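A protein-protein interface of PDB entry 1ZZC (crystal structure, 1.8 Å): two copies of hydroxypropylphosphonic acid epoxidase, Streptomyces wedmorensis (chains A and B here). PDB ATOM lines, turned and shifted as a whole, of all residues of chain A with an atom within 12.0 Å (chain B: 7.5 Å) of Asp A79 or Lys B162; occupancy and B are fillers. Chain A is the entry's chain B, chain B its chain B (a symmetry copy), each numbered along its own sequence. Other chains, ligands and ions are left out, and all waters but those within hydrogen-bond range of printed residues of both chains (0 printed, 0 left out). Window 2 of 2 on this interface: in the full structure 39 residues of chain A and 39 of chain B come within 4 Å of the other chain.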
ATOM      1  N   GLY A  75      -4.745  24.257  26.646  1.00  0.00           N
ATOM      2  CA  GLY A  75      -4.428  25.182  25.574  1.00  0.00           C
ATOM      3  C   GLY A  75      -4.775  24.651  24.188  1.00  0.00           C
ATOM      4  O   GLY A  75      -5.324  23.545  24.040  1.00  0.00           O
ATOM      5  N   ASN A  76      -4.481  25.452  23.170  1.00  0.00           N
ATOM      6  CA  ASN A  76      -4.788  25.060  21.807  1.00  0.00           C
ATOM      7  C   ASN A  76      -3.564  25.110  20.922  1.00  0.00           C
ATOM      8  O   ASN A  76      -2.973  26.170  20.710  1.00  0.00           O
ATOM      9  CB  ASN A  76      -5.877  25.957  21.226  1.00  0.00           C
ATOM     10  CG  ASN A  76      -6.530  25.347  20.007  1.00  0.00           C
ATOM     11  OD1 ASN A  76      -5.843  24.883  19.083  1.00  0.00           O
ATOM     12  ND2 ASN A  76      -7.866  25.343  19.991  1.00  0.00           N
ATOM     13  N   ASP A  77      -3.183  23.947  20.410  1.00  0.00           N
ATOM     14  CA  ASP A  77      -2.023  23.815  19.544  1.00  0.00           C
ATOM     15  C   ASP A  77      -2.412  23.348  18.134  1.00  0.00           C
ATOM     16  O   ASP A  77      -1.573  22.858  17.373  1.00  0.00           O
ATOM     17  CB  ASP A  77      -1.030  22.822  20.164  1.00  0.00           C
ATOM     18  CG  ASP A  77      -1.681  21.487  20.551  1.00  0.00           C
ATOM     19  OD1 ASP A  77      -2.877  21.253  20.233  1.00  0.00           O
ATOM     20  OD2 ASP A  77      -0.977  20.655  21.173  1.00  0.00           O
ATOM     21  N   LEU A  78      -3.687  23.524  17.800  1.00  0.00           N
ATOM     22  CA  LEU A  78      -4.223  23.114  16.514  1.00  0.00           C
ATOM     23  C   LEU A  78      -4.153  24.205  15.462  1.00  0.00           C
ATOM     24  O   LEU A  78      -4.089  25.401  15.781  1.00  0.00           O
ATOM     25  CB  LEU A  78      -5.682  22.669  16.679  1.00  0.00           C
ATOM     26  CG  LEU A  78      -5.938  21.577  17.728  1.00  0.00           C
ATOM     27  CD1 LEU A  78      -7.428  21.222  17.789  1.00  0.00           C
ATOM     28  CD2 LEU A  78      -5.100  20.346  17.389  1.00  0.00           C
ATOM     29  N   ASP A  79      -4.178  23.788  14.199  1.00  0.00           N
ATOM     30  CA  ASP A  79      -4.152  24.720  13.088  1.00  0.00           C
ATOM     31  C   ASP A  79      -5.515  24.553  12.434  1.00  0.00           C
ATOM     32  O   ASP A  79      -5.741  23.617  11.657  1.00  0.00           O
ATOM     33  CB  ASP A  79      -3.024  24.379  12.107  1.00  0.00           C
ATOM     34  CG  ASP A  79      -3.167  25.116  10.763  1.00  0.00           C
ATOM     35  OD1 ASP A  79      -3.958  26.082  10.690  1.00  0.00           O
ATOM     36  OD2 ASP A  79      -2.501  24.735   9.788  1.00  0.00           O
ATOM     37  N   ASP A  80      -6.431  25.455  12.777  1.00  0.00           N
ATOM     38  CA  ASP A  80      -7.800  25.395  12.267  1.00  0.00           C
ATOM     39  C   ASP A  80      -8.386  24.015  12.586  1.00  0.00           C
ATOM     40  O   ASP A  80      -9.013  23.372  11.740  1.00  0.00           O
ATOM     41  CB  ASP A  80      -7.825  25.661  10.741  1.00  0.00           C
ATOM     42  N   GLY A  81      -8.118  23.540  13.804  1.00  0.00           N
ATOM     43  CA  GLY A  81      -8.692  22.280  14.258  1.00  0.00           C
ATOM     44  C   GLY A  81      -7.943  20.987  13.975  1.00  0.00           C
ATOM     45  O   GLY A  81      -8.447  19.898  14.290  1.00  0.00           O
ATOM     46  N   VAL A  82      -6.743  21.099  13.419  1.00  0.00           N
ATOM     47  CA  VAL A  82      -5.965  19.916  13.060  1.00  0.00           C
ATOM     48  C   VAL A  82      -4.507  19.997  13.479  1.00  0.00           C
ATOM     49  O   VAL A  82      -3.930  21.079  13.553  1.00  0.00           O
ATOM     50  CB  VAL A  82      -6.007  19.712  11.511  1.00  0.00           C
ATOM     51  CG1 VAL A  82      -5.095  18.571  11.090  1.00  0.00           C
ATOM     52  CG2 VAL A  82      -7.437  19.474  11.070  1.00  0.00           C
ATOM     53  N   ILE A  83      -3.906  18.862  13.793  1.00  0.00           N
ATOM     54  CA  ILE A  83      -2.483  18.873  14.080  1.00  0.00           C
ATOM     55  C   ILE A  83      -1.941  17.637  13.384  1.00  0.00           C
ATOM     56  O   ILE A  83      -2.533  16.543  13.478  1.00  0.00           O
ATOM     57  CB  ILE A  83      -2.136  18.871  15.611  1.00  0.00           C
ATOM     58  CG1 ILE A  83      -0.614  18.949  15.765  1.00  0.00           C
ATOM     59  CG2 ILE A  83      -2.671  17.602  16.326  1.00  0.00           C
ATOM     60  CD1 ILE A  83      -0.121  19.263  17.190  1.00  0.00           C
ATOM     61  N   ILE A  84      -0.847  17.809  12.644  1.00  0.00           N
ATOM     62  CA  ILE A  84      -0.265  16.671  11.932  1.00  0.00           C
ATOM     63  C   ILE A  84       1.169  16.412  12.358  1.00  0.00           C
ATOM     64  O   ILE A  84       1.859  17.307  12.857  1.00  0.00           O
ATOM     65  CB  ILE A  84      -0.339  16.848  10.366  1.00  0.00           C
ATOM     66  CG1 ILE A  84       0.645  17.908   9.870  1.00  0.00           C
ATOM     67  CG2 ILE A  84      -1.759  17.193   9.934  1.00  0.00           C
ATOM     68  CD1 ILE A  84       2.009  17.342   9.530  1.00  0.00           C
ATOM     69  N   GLN A  85       1.601  15.164  12.201  1.00  0.00           N
ATOM     70  CA  GLN A  85       2.962  14.786  12.529  1.00  0.00           C
ATOM     71  C   GLN A  85       3.558  13.945  11.402  1.00  0.00           C
ATOM     72  O   GLN A  85       3.045  12.867  11.060  1.00  0.00           O
ATOM     73  CB  GLN A  85       3.032  14.000  13.828  1.00  0.00           C
ATOM     74  CG  GLN A  85       4.446  13.483  14.120  1.00  0.00           C
ATOM     75  CD  GLN A  85       4.556  12.777  15.457  1.00  0.00           C
ATOM     76  OE1 GLN A  85       4.615  13.416  16.490  1.00  0.00           O
ATOM     77  NE2 GLN A  85       4.563  11.457  15.437  1.00  0.00           N
ATOM     78  N   VAL A 109       1.380  11.664  16.838  1.00  0.00           N
ATOM     79  CA  VAL A 109       0.823  12.980  17.164  1.00  0.00           C
ATOM     80  C   VAL A 109       0.012  13.046  18.463  1.00  0.00           C
ATOM     81  O   VAL A 109      -0.732  12.130  18.785  1.00  0.00           O
ATOM     82  CB  VAL A 109      -0.044  13.512  15.967  1.00  0.00           C
ATOM     83  CG1 VAL A 109      -1.414  12.781  15.912  1.00  0.00           C
ATOM     84  CG2 VAL A 109      -0.250  15.026  16.086  1.00  0.00           C
ATOM     85  N   ARG A 110       0.208  14.131  19.225  1.00  0.00           N
ATOM     86  CA  ARG A 110      -0.548  14.371  20.451  1.00  0.00           C
ATOM     87  C   ARG A 110      -1.043  15.824  20.399  1.00  0.00           C
ATOM     88  O   ARG A 110      -0.576  16.645  19.598  1.00  0.00           O
ATOM     89  CB  ARG A 110       0.320  14.154  21.706  1.00  0.00           C
ATOM     90  CG  ARG A 110       0.749  12.704  21.910  1.00  0.00           C
ATOM     91  CD  ARG A 110       1.198  12.461  23.344  1.00  0.00           C
ATOM     92  NE  ARG A 110       2.396  13.238  23.715  1.00  0.00           N
ATOM     93  CZ  ARG A 110       3.648  12.783  23.652  1.00  0.00           C
ATOM     94  NH1 ARG A 110       4.666  13.559  24.023  1.00  0.00           N
ATOM     95  NH2 ARG A 110       3.894  11.553  23.218  1.00  0.00           N
ATOM     96  N   THR A 111      -1.992  16.149  21.255  1.00  0.00           N
ATOM     97  CA  THR A 111      -2.519  17.510  21.254  1.00  0.00           C
ATOM     98  C   THR A 111      -3.027  17.891  22.623  1.00  0.00           C
ATOM     99  O   THR A 111      -3.642  17.079  23.315  1.00  0.00           O
ATOM    100  CB  THR A 111      -3.680  17.661  20.215  1.00  0.00           C
ATOM    101  OG1 THR A 111      -4.355  18.931  20.389  1.00  0.00           O
ATOM    102  CG2 THR A 111      -4.681  16.508  20.390  1.00  0.00           C
ATOM    103  N   LYS A 112      -2.755  19.138  23.008  1.00  0.00           N
ATOM    104  CA  LYS A 112      -3.218  19.643  24.297  1.00  0.00           C
ATOM    105  C   LYS A 112      -4.744  19.744  24.305  1.00  0.00           C
ATOM    106  O   LYS A 112      -5.355  19.928  25.365  1.00  0.00           O
ATOM    107  CB  LYS A 112      -2.595  21.027  24.582  1.00  0.00           C
ATOM    108  CG  LYS A 112      -1.119  20.942  24.891  1.00  0.00           C
ATOM    109  CD  LYS A 112      -0.547  22.204  25.536  1.00  0.00           C
ATOM    110  CE  LYS A 112      -0.494  23.373  24.579  1.00  0.00           C
ATOM    111  NZ  LYS A 112       0.205  24.505  25.257  1.00  0.00           N
ATOM    112  N   ARG A 113      -5.365  19.634  23.133  1.00  0.00           N
ATOM    113  CA  ARG A 113      -6.832  19.698  23.079  1.00  0.00           C
ATOM    114  C   ARG A 113      -7.500  18.372  23.440  1.00  0.00           C
ATOM    115  O   ARG A 113      -8.721  18.314  23.636  1.00  0.00           O
ATOM    116  CB  ARG A 113      -7.299  20.200  21.706  1.00  0.00           C
ATOM    117  CG  ARG A 113      -6.904  21.655  21.471  1.00  0.00           C
ATOM    118  CD  ARG A 113      -7.826  22.652  22.205  1.00  0.00           C
ATOM    119  NE  ARG A 113      -9.141  22.746  21.557  1.00  0.00           N
ATOM    120  CZ  ARG A 113     -10.071  23.661  21.840  1.00  0.00           C
ATOM    121  NH1 ARG A 113      -9.851  24.588  22.768  1.00  0.00           N
ATOM    122  NH2 ARG A 113     -11.235  23.647  21.191  1.00  0.00           N
ATOM    123  N   ALA A 114      -6.696  17.313  23.557  1.00  0.00           N
ATOM    124  CA  ALA A 114      -7.192  15.995  23.950  1.00  0.00           C
ATOM    125  C   ALA A 114      -6.001  15.343  24.635  1.00  0.00           C
ATOM    126  O   ALA A 114      -5.419  14.372  24.141  1.00  0.00           O
ATOM    127  CB  ALA A 114      -7.630  15.184  22.717  1.00  0.00           C
ATOM    128  N   PHE B 134     -15.865  16.806   1.250  1.00  0.00           N
ATOM    129  CA  PHE B 134     -15.760  17.054   2.683  1.00  0.00           C
ATOM    130  C   PHE B 134     -16.788  16.490   3.653  1.00  0.00           C
ATOM    131  O   PHE B 134     -17.986  16.745   3.507  1.00  0.00           O
ATOM    132  CB  PHE B 134     -15.706  18.560   2.946  1.00  0.00           C
ATOM    133  CG  PHE B 134     -14.414  19.203   2.558  1.00  0.00           C
ATOM    134  CD1 PHE B 134     -14.034  19.288   1.221  1.00  0.00           C
ATOM    135  CD2 PHE B 134     -13.582  19.751   3.532  1.00  0.00           C
ATOM    136  CE1 PHE B 134     -12.840  19.914   0.863  1.00  0.00           C
ATOM    137  CE2 PHE B 134     -12.386  20.379   3.186  1.00  0.00           C
ATOM    138  CZ  PHE B 134     -12.019  20.461   1.843  1.00  0.00           C
ATOM    139  N   HIS B 152      -3.550  13.019   0.549  1.00  0.00           N
ATOM    140  CA  HIS B 152      -3.694  14.448   0.362  1.00  0.00           C
ATOM    141  C   HIS B 152      -4.895  14.801   1.228  1.00  0.00           C
ATOM    142  O   HIS B 152      -6.047  14.493   0.906  1.00  0.00           O
ATOM    143  CB  HIS B 152      -3.975  14.807  -1.094  1.00  0.00           C
ATOM    144  CG  HIS B 152      -3.983  16.281  -1.345  1.00  0.00           C
ATOM    145  ND1 HIS B 152      -3.310  16.861  -2.396  1.00  0.00           N
ATOM    146  CD2 HIS B 152      -4.589  17.293  -0.680  1.00  0.00           C
ATOM    147  CE1 HIS B 152      -3.501  18.169  -2.369  1.00  0.00           C
ATOM    148  NE2 HIS B 152      -4.276  18.456  -1.340  1.00  0.00           N
ATOM    149  N   MET B 153      -4.619  15.408   2.369  1.00  0.00           N
ATOM    150  CA  MET B 153      -5.679  15.777   3.278  1.00  0.00           C
ATOM    151  C   MET B 153      -6.068  17.237   3.111  1.00  0.00           C
ATOM    152  O   MET B 153      -5.223  18.071   2.809  1.00  0.00           O
ATOM    153  CB  MET B 153      -5.219  15.510   4.719  1.00  0.00           C
ATOM    154  CG  MET B 153      -6.099  16.112   5.793  1.00  0.00           C
ATOM    155  SD  MET B 153      -5.411  15.725   7.427  1.00  0.00           S
ATOM    156  CE  MET B 153      -6.831  16.055   8.545  1.00  0.00           C
ATOM    157  N   LYS B 154      -7.350  17.529   3.305  1.00  0.00           N
ATOM    158  CA  LYS B 154      -7.847  18.908   3.245  1.00  0.00           C
ATOM    159  C   LYS B 154      -8.782  19.106   4.427  1.00  0.00           C
ATOM    160  O   LYS B 154      -9.489  18.180   4.832  1.00  0.00           O
ATOM    161  CB  LYS B 154      -8.627  19.184   1.950  1.00  0.00           C
ATOM    162  CG  LYS B 154      -7.834  18.996   0.659  1.00  0.00           C
ATOM    163  CD  LYS B 154      -8.736  19.307  -0.545  1.00  0.00           C
ATOM    164  CE  LYS B 154      -7.987  19.168  -1.857  1.00  0.00           C
ATOM    165  NZ  LYS B 154      -8.799  19.712  -2.974  1.00  0.00           N
ATOM    166  N   TRP B 155      -8.796  20.304   4.991  1.00  0.00           N
ATOM    167  CA  TRP B 155      -9.683  20.544   6.109  1.00  0.00           C
ATOM    168  C   TRP B 155      -9.993  22.013   6.251  1.00  0.00           C
ATOM    169  O   TRP B 155      -9.425  22.839   5.549  1.00  0.00           O
ATOM    170  CB  TRP B 155      -9.075  19.999   7.417  1.00  0.00           C
ATOM    171  CG  TRP B 155      -7.930  20.794   7.994  1.00  0.00           C
ATOM    172  CD1 TRP B 155      -7.999  21.797   8.941  1.00  0.00           C
ATOM    173  CD2 TRP B 155      -6.539  20.577   7.746  1.00  0.00           C
ATOM    174  NE1 TRP B 155      -6.730  22.199   9.294  1.00  0.00           N
ATOM    175  CE2 TRP B 155      -5.818  21.467   8.578  1.00  0.00           C
ATOM    176  CE3 TRP B 155      -5.828  19.710   6.901  1.00  0.00           C
ATOM    177  CZ2 TRP B 155      -4.418  21.513   8.589  1.00  0.00           C
ATOM    178  CZ3 TRP B 155      -4.438  19.757   6.910  1.00  0.00           C
ATOM    179  CH2 TRP B 155      -3.746  20.655   7.753  1.00  0.00           C
ATOM    180  N   GLY B 156     -10.908  22.315   7.166  1.00  0.00           N
ATOM    181  CA  GLY B 156     -11.299  23.694   7.406  1.00  0.00           C
ATOM    182  C   GLY B 156     -12.368  24.127   6.418  1.00  0.00           C
ATOM    183  O   GLY B 156     -13.360  23.429   6.219  1.00  0.00           O
ATOM    184  N   ASP B 157     -12.157  25.278   5.790  1.00  0.00           N
ATOM    185  CA  ASP B 157     -13.104  25.819   4.820  1.00  0.00           C
ATOM    186  C   ASP B 157     -13.001  25.152   3.444  1.00  0.00           C
ATOM    187  O   ASP B 157     -11.985  25.287   2.743  1.00  0.00           O
ATOM    188  CB  ASP B 157     -12.864  27.318   4.688  1.00  0.00           C
ATOM    189  CG  ASP B 157     -13.657  27.935   3.562  1.00  0.00           C
ATOM    190  OD1 ASP B 157     -13.228  29.009   3.084  1.00  0.00           O
ATOM    191  OD2 ASP B 157     -14.691  27.360   3.166  1.00  0.00           O
ATOM    192  N   LYS B 158     -14.063  24.449   3.053  1.00  0.00           N
ATOM    193  CA  LYS B 158     -14.091  23.747   1.769  1.00  0.00           C
ATOM    194  C   LYS B 158     -13.679  24.631   0.584  1.00  0.00           C
ATOM    195  O   LYS B 158     -13.136  24.128  -0.408  1.00  0.00           O
ATOM    196  CB  LYS B 158     -15.498  23.172   1.505  1.00  0.00           C
ATOM    197  CG  LYS B 158     -16.575  24.232   1.323  1.00  0.00           C
ATOM    198  CD  LYS B 158     -17.821  23.714   0.575  1.00  0.00           C
ATOM    199  CE  LYS B 158     -18.600  22.674   1.364  1.00  0.00           C
ATOM    200  NZ  LYS B 158     -19.878  22.272   0.658  1.00  0.00           N
ATOM    201  N   ASN B 160     -11.469  27.324   0.724  1.00  0.00           N
ATOM    202  CA  ASN B 160     -10.079  27.774   0.815  1.00  0.00           C
ATOM    203  C   ASN B 160      -9.561  26.955   1.993  1.00  0.00           C
ATOM    204  O   ASN B 160      -9.329  27.475   3.086  1.00  0.00           O
ATOM    205  CB  ASN B 160     -10.044  29.269   1.129  1.00  0.00           C
ATOM    206  CG  ASN B 160      -8.633  29.805   1.263  1.00  0.00           C
ATOM    207  OD1 ASN B 160      -7.734  29.427   0.506  1.00  0.00           O
ATOM    208  ND2 ASN B 160      -8.434  30.705   2.219  1.00  0.00           N
ATOM    209  N   PRO B 161      -9.394  25.646   1.781  1.00  0.00           N
ATOM    210  CA  PRO B 161      -8.929  24.744   2.834  1.00  0.00           C
ATOM    211  C   PRO B 161      -7.452  24.704   3.167  1.00  0.00           C
ATOM    212  O   PRO B 161      -6.588  25.123   2.389  1.00  0.00           O
ATOM    213  CB  PRO B 161      -9.413  23.382   2.343  1.00  0.00           C
ATOM    214  CG  PRO B 161      -9.170  23.488   0.866  1.00  0.00           C
ATOM    215  CD  PRO B 161      -9.657  24.904   0.530  1.00  0.00           C
ATOM    216  N   LYS B 162      -7.196  24.190   4.364  1.00  0.00           N
ATOM    217  CA  LYS B 162      -5.850  23.961   4.834  1.00  0.00           C
ATOM    218  C   LYS B 162      -5.596  22.608   4.164  1.00  0.00           C
ATOM    219  O   LYS B 162      -6.550  21.846   3.897  1.00  0.00           O
ATOM    220  CB  LYS B 162      -5.829  23.802   6.355  1.00  0.00           C
ATOM    221  CG  LYS B 162      -6.168  25.063   7.142  1.00  0.00           C
ATOM    222  CD  LYS B 162      -5.329  26.259   6.703  1.00  0.00           C
ATOM    223  CE  LYS B 162      -3.842  25.949   6.768  1.00  0.00           C
ATOM    224  NZ  LYS B 162      -2.983  27.017   6.180  1.00  0.00           N
ATOM    225  N   GLU B 163      -4.332  22.307   3.880  1.00  0.00           N
ATOM    226  CA  GLU B 163      -3.985  21.061   3.204  1.00  0.00           C
ATOM    227  C   GLU B 163      -2.673  20.483   3.692  1.00  0.00           C
ATOM    228  O   GLU B 163      -1.834  21.194   4.261  1.00  0.00           O
ATOM    229  CB  GLU B 163      -3.853  21.292   1.693  1.00  0.00           C
ATOM    230  CG  GLU B 163      -5.014  22.004   1.044  1.00  0.00           C
ATOM    231  CD  GLU B 163      -4.804  22.140  -0.454  1.00  0.00           C
ATOM    232  OE1 GLU B 163      -5.044  21.152  -1.178  1.00  0.00           O
ATOM    233  OE2 GLU B 163      -4.358  23.214  -0.904  1.00  0.00           O
ATOM    234  N   ALA B 164      -2.488  19.193   3.427  1.00  0.00           N
ATOM    235  CA  ALA B 164      -1.276  18.506   3.811  1.00  0.00           C
ATOM    236  C   ALA B 164      -1.092  17.219   3.005  1.00  0.00           C
ATOM    237  O   ALA B 164      -2.050  16.465   2.815  1.00  0.00           O
ATOM    238  CB  ALA B 164      -1.315  18.180   5.310  1.00  0.00           C
ATOM    239  N   PHE B 173      -4.592  14.507  13.903  1.00  0.00           N
ATOM    240  CA  PHE B 173      -5.668  14.593  14.875  1.00  0.00           C
ATOM    241  C   PHE B 173      -6.614  15.624  14.300  1.00  0.00           C
ATOM    242  O   PHE B 173      -6.170  16.690  13.836  1.00  0.00           O
ATOM    243  CB  PHE B 173      -5.154  15.101  16.219  1.00  0.00           C
ATOM    244  CG  PHE B 173      -6.248  15.509  17.156  1.00  0.00           C
ATOM    245  CD1 PHE B 173      -6.874  14.574  17.965  1.00  0.00           C
ATOM    246  CD2 PHE B 173      -6.661  16.848  17.216  1.00  0.00           C
ATOM    247  CE1 PHE B 173      -7.907  14.952  18.841  1.00  0.00           C
ATOM    248  CE2 PHE B 173      -7.680  17.237  18.074  1.00  0.00           C
ATOM    249  CZ  PHE B 173      -8.304  16.287  18.892  1.00  0.00           C
ATOM    250  N   VAL B 178     -14.707  19.729  12.813  1.00  0.00           N
ATOM    251  CA  VAL B 178     -13.844  20.301  11.799  1.00  0.00           C
ATOM    252  C   VAL B 178     -14.056  19.506  10.508  1.00  0.00           C
ATOM    253  O   VAL B 178     -13.852  18.293  10.486  1.00  0.00           O
ATOM    254  CB  VAL B 178     -12.351  20.223  12.215  1.00  0.00           C
ATOM    255  CG1 VAL B 178     -11.473  20.735  11.095  1.00  0.00           C
ATOM    256  CG2 VAL B 178     -12.120  21.056  13.491  1.00  0.00           C
ATOM    257  N   PRO B 179     -14.504  20.170   9.431  1.00  0.00           N
ATOM    258  CA  PRO B 179     -14.722  19.468   8.161  1.00  0.00           C
ATOM    259  C   PRO B 179     -13.389  18.992   7.569  1.00  0.00           C
ATOM    260  O   PRO B 179     -12.367  19.677   7.686  1.00  0.00           O
ATOM    261  CB  PRO B 179     -15.448  20.507   7.290  1.00  0.00           C
ATOM    262  CG  PRO B 179     -15.088  21.836   7.904  1.00  0.00           C
ATOM    263  CD  PRO B 179     -15.005  21.563   9.384  1.00  0.00           C
ATOM    264  N   ALA B 181     -11.471  16.148   4.383  1.00  0.00           N
ATOM    265  CA  ALA B 181     -11.583  15.240   3.241  1.00  0.00           C
ATOM    266  C   ALA B 181     -10.214  14.637   2.931  1.00  0.00           C
ATOM    267  O   ALA B 181      -9.180  15.187   3.317  1.00  0.00           O
ATOM    268  CB  ALA B 181     -12.113  16.005   2.031  1.00  0.00           C
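The indole nitrogen (NE1) of Trp B155 sits at hydrogen-bond distance from the backbone carbonyl oxygen (O) of Asp A79, at 2.9 Å. The backbone carbonyl oxygen of Ile A83 is in hydrogen-bond range of the backbone NH of Phe B173.
N of Met B153 sits at hydrogen-bond distance from O of Ala B164, at 2.8 Å. The side-chain hydroxyl (OG1) of Thr A111 sits close to the backbone NH (N) of Arg A113, at 3.0 Å. The side-chain amide oxygen of Asn A76 lies within hydrogen-bond range of the backbone NH of Leu A78, at 2.9 Å. O of Trp B155 lies within hydrogen-bond range of N of Lys B162, at 2.9 Å. OG1 of Thr A111 is in hydrogen-bond range of OD1 of Asp A77, 2.8 Å away.
Among the printed residues, pairs that only touch across the chains: Val A82 with Trp B155 (3.2 Å), Val A82 with Phe B173 (3.3 Å), Asp A80 with Trp B155 (3.4 Å), Asp A79 with Lys B162 (3.5 Å), Asp A80 with Val B178 (3.7 Å), Gly A81 with Val B178 (3.7 Å), Thr A111 with Phe B173 (3.7 Å), Leu A78 with Phe B173 (3.8 Å), Ala A114 with Phe B173 (3.9 Å), Gly A81 with Phe B173 (3.96 Å) and Val A82 with Met B153 (3.98 Å).
Of chain B, only Trp B155 and Lys B162 come within 4 Å of Asp A79. Printed residues of chain A within 4 Å of Lys B162: Asp A79 (3.5 Å). Printed residues of chain A within 4 Å of Met B153: Val A82 (3.98 Å). Trp B155 touches three residues of chain A. No residue of chain A comes within 4 Å of Asn B160. Pro B161 touches none of the printed residues of chain A. No residue of chain A comes within 4 Å of Glu B163. Ala B164 touches none of the printed residues of chain A. Of the printed residues of chain B, Leu A78 touches Phe B173. Of the printed residues of chain A, Phe B173 touches Leu A78, Gly A81, Val A82, Ile A83, Thr A111 and Ala A114. Of the printed residues of chain B, Asp A80 touches Trp B155 (3.4 Å) and Val B178 (3.7 Å). Asp B157 touches none of the printed residues of chain A. Val A109 touches none of the printed residues of chain B. The nearest printed residue of chain A that does not touch Lys B162 is Asp A80 (4.01 Å). The nearest printed residue of chain B that does not touch Gly A81 is Trp B155 (4.9 Å).
Printed residues of chain B that touch a printed residue of chain A: Met B153, Trp B155, Lys B162, Phe B173 and Val B178. Hydrophobic or aromatic side chains of chain A that line the printed part of chain B: Leu A78, Val A82, Ile A83 and Ala A114. Among the printed residues, no Asp or Glu carboxylate lies within 4 Å of a Lys or Arg side-chain nitrogen of the other chain.
No position is printed for both chains.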
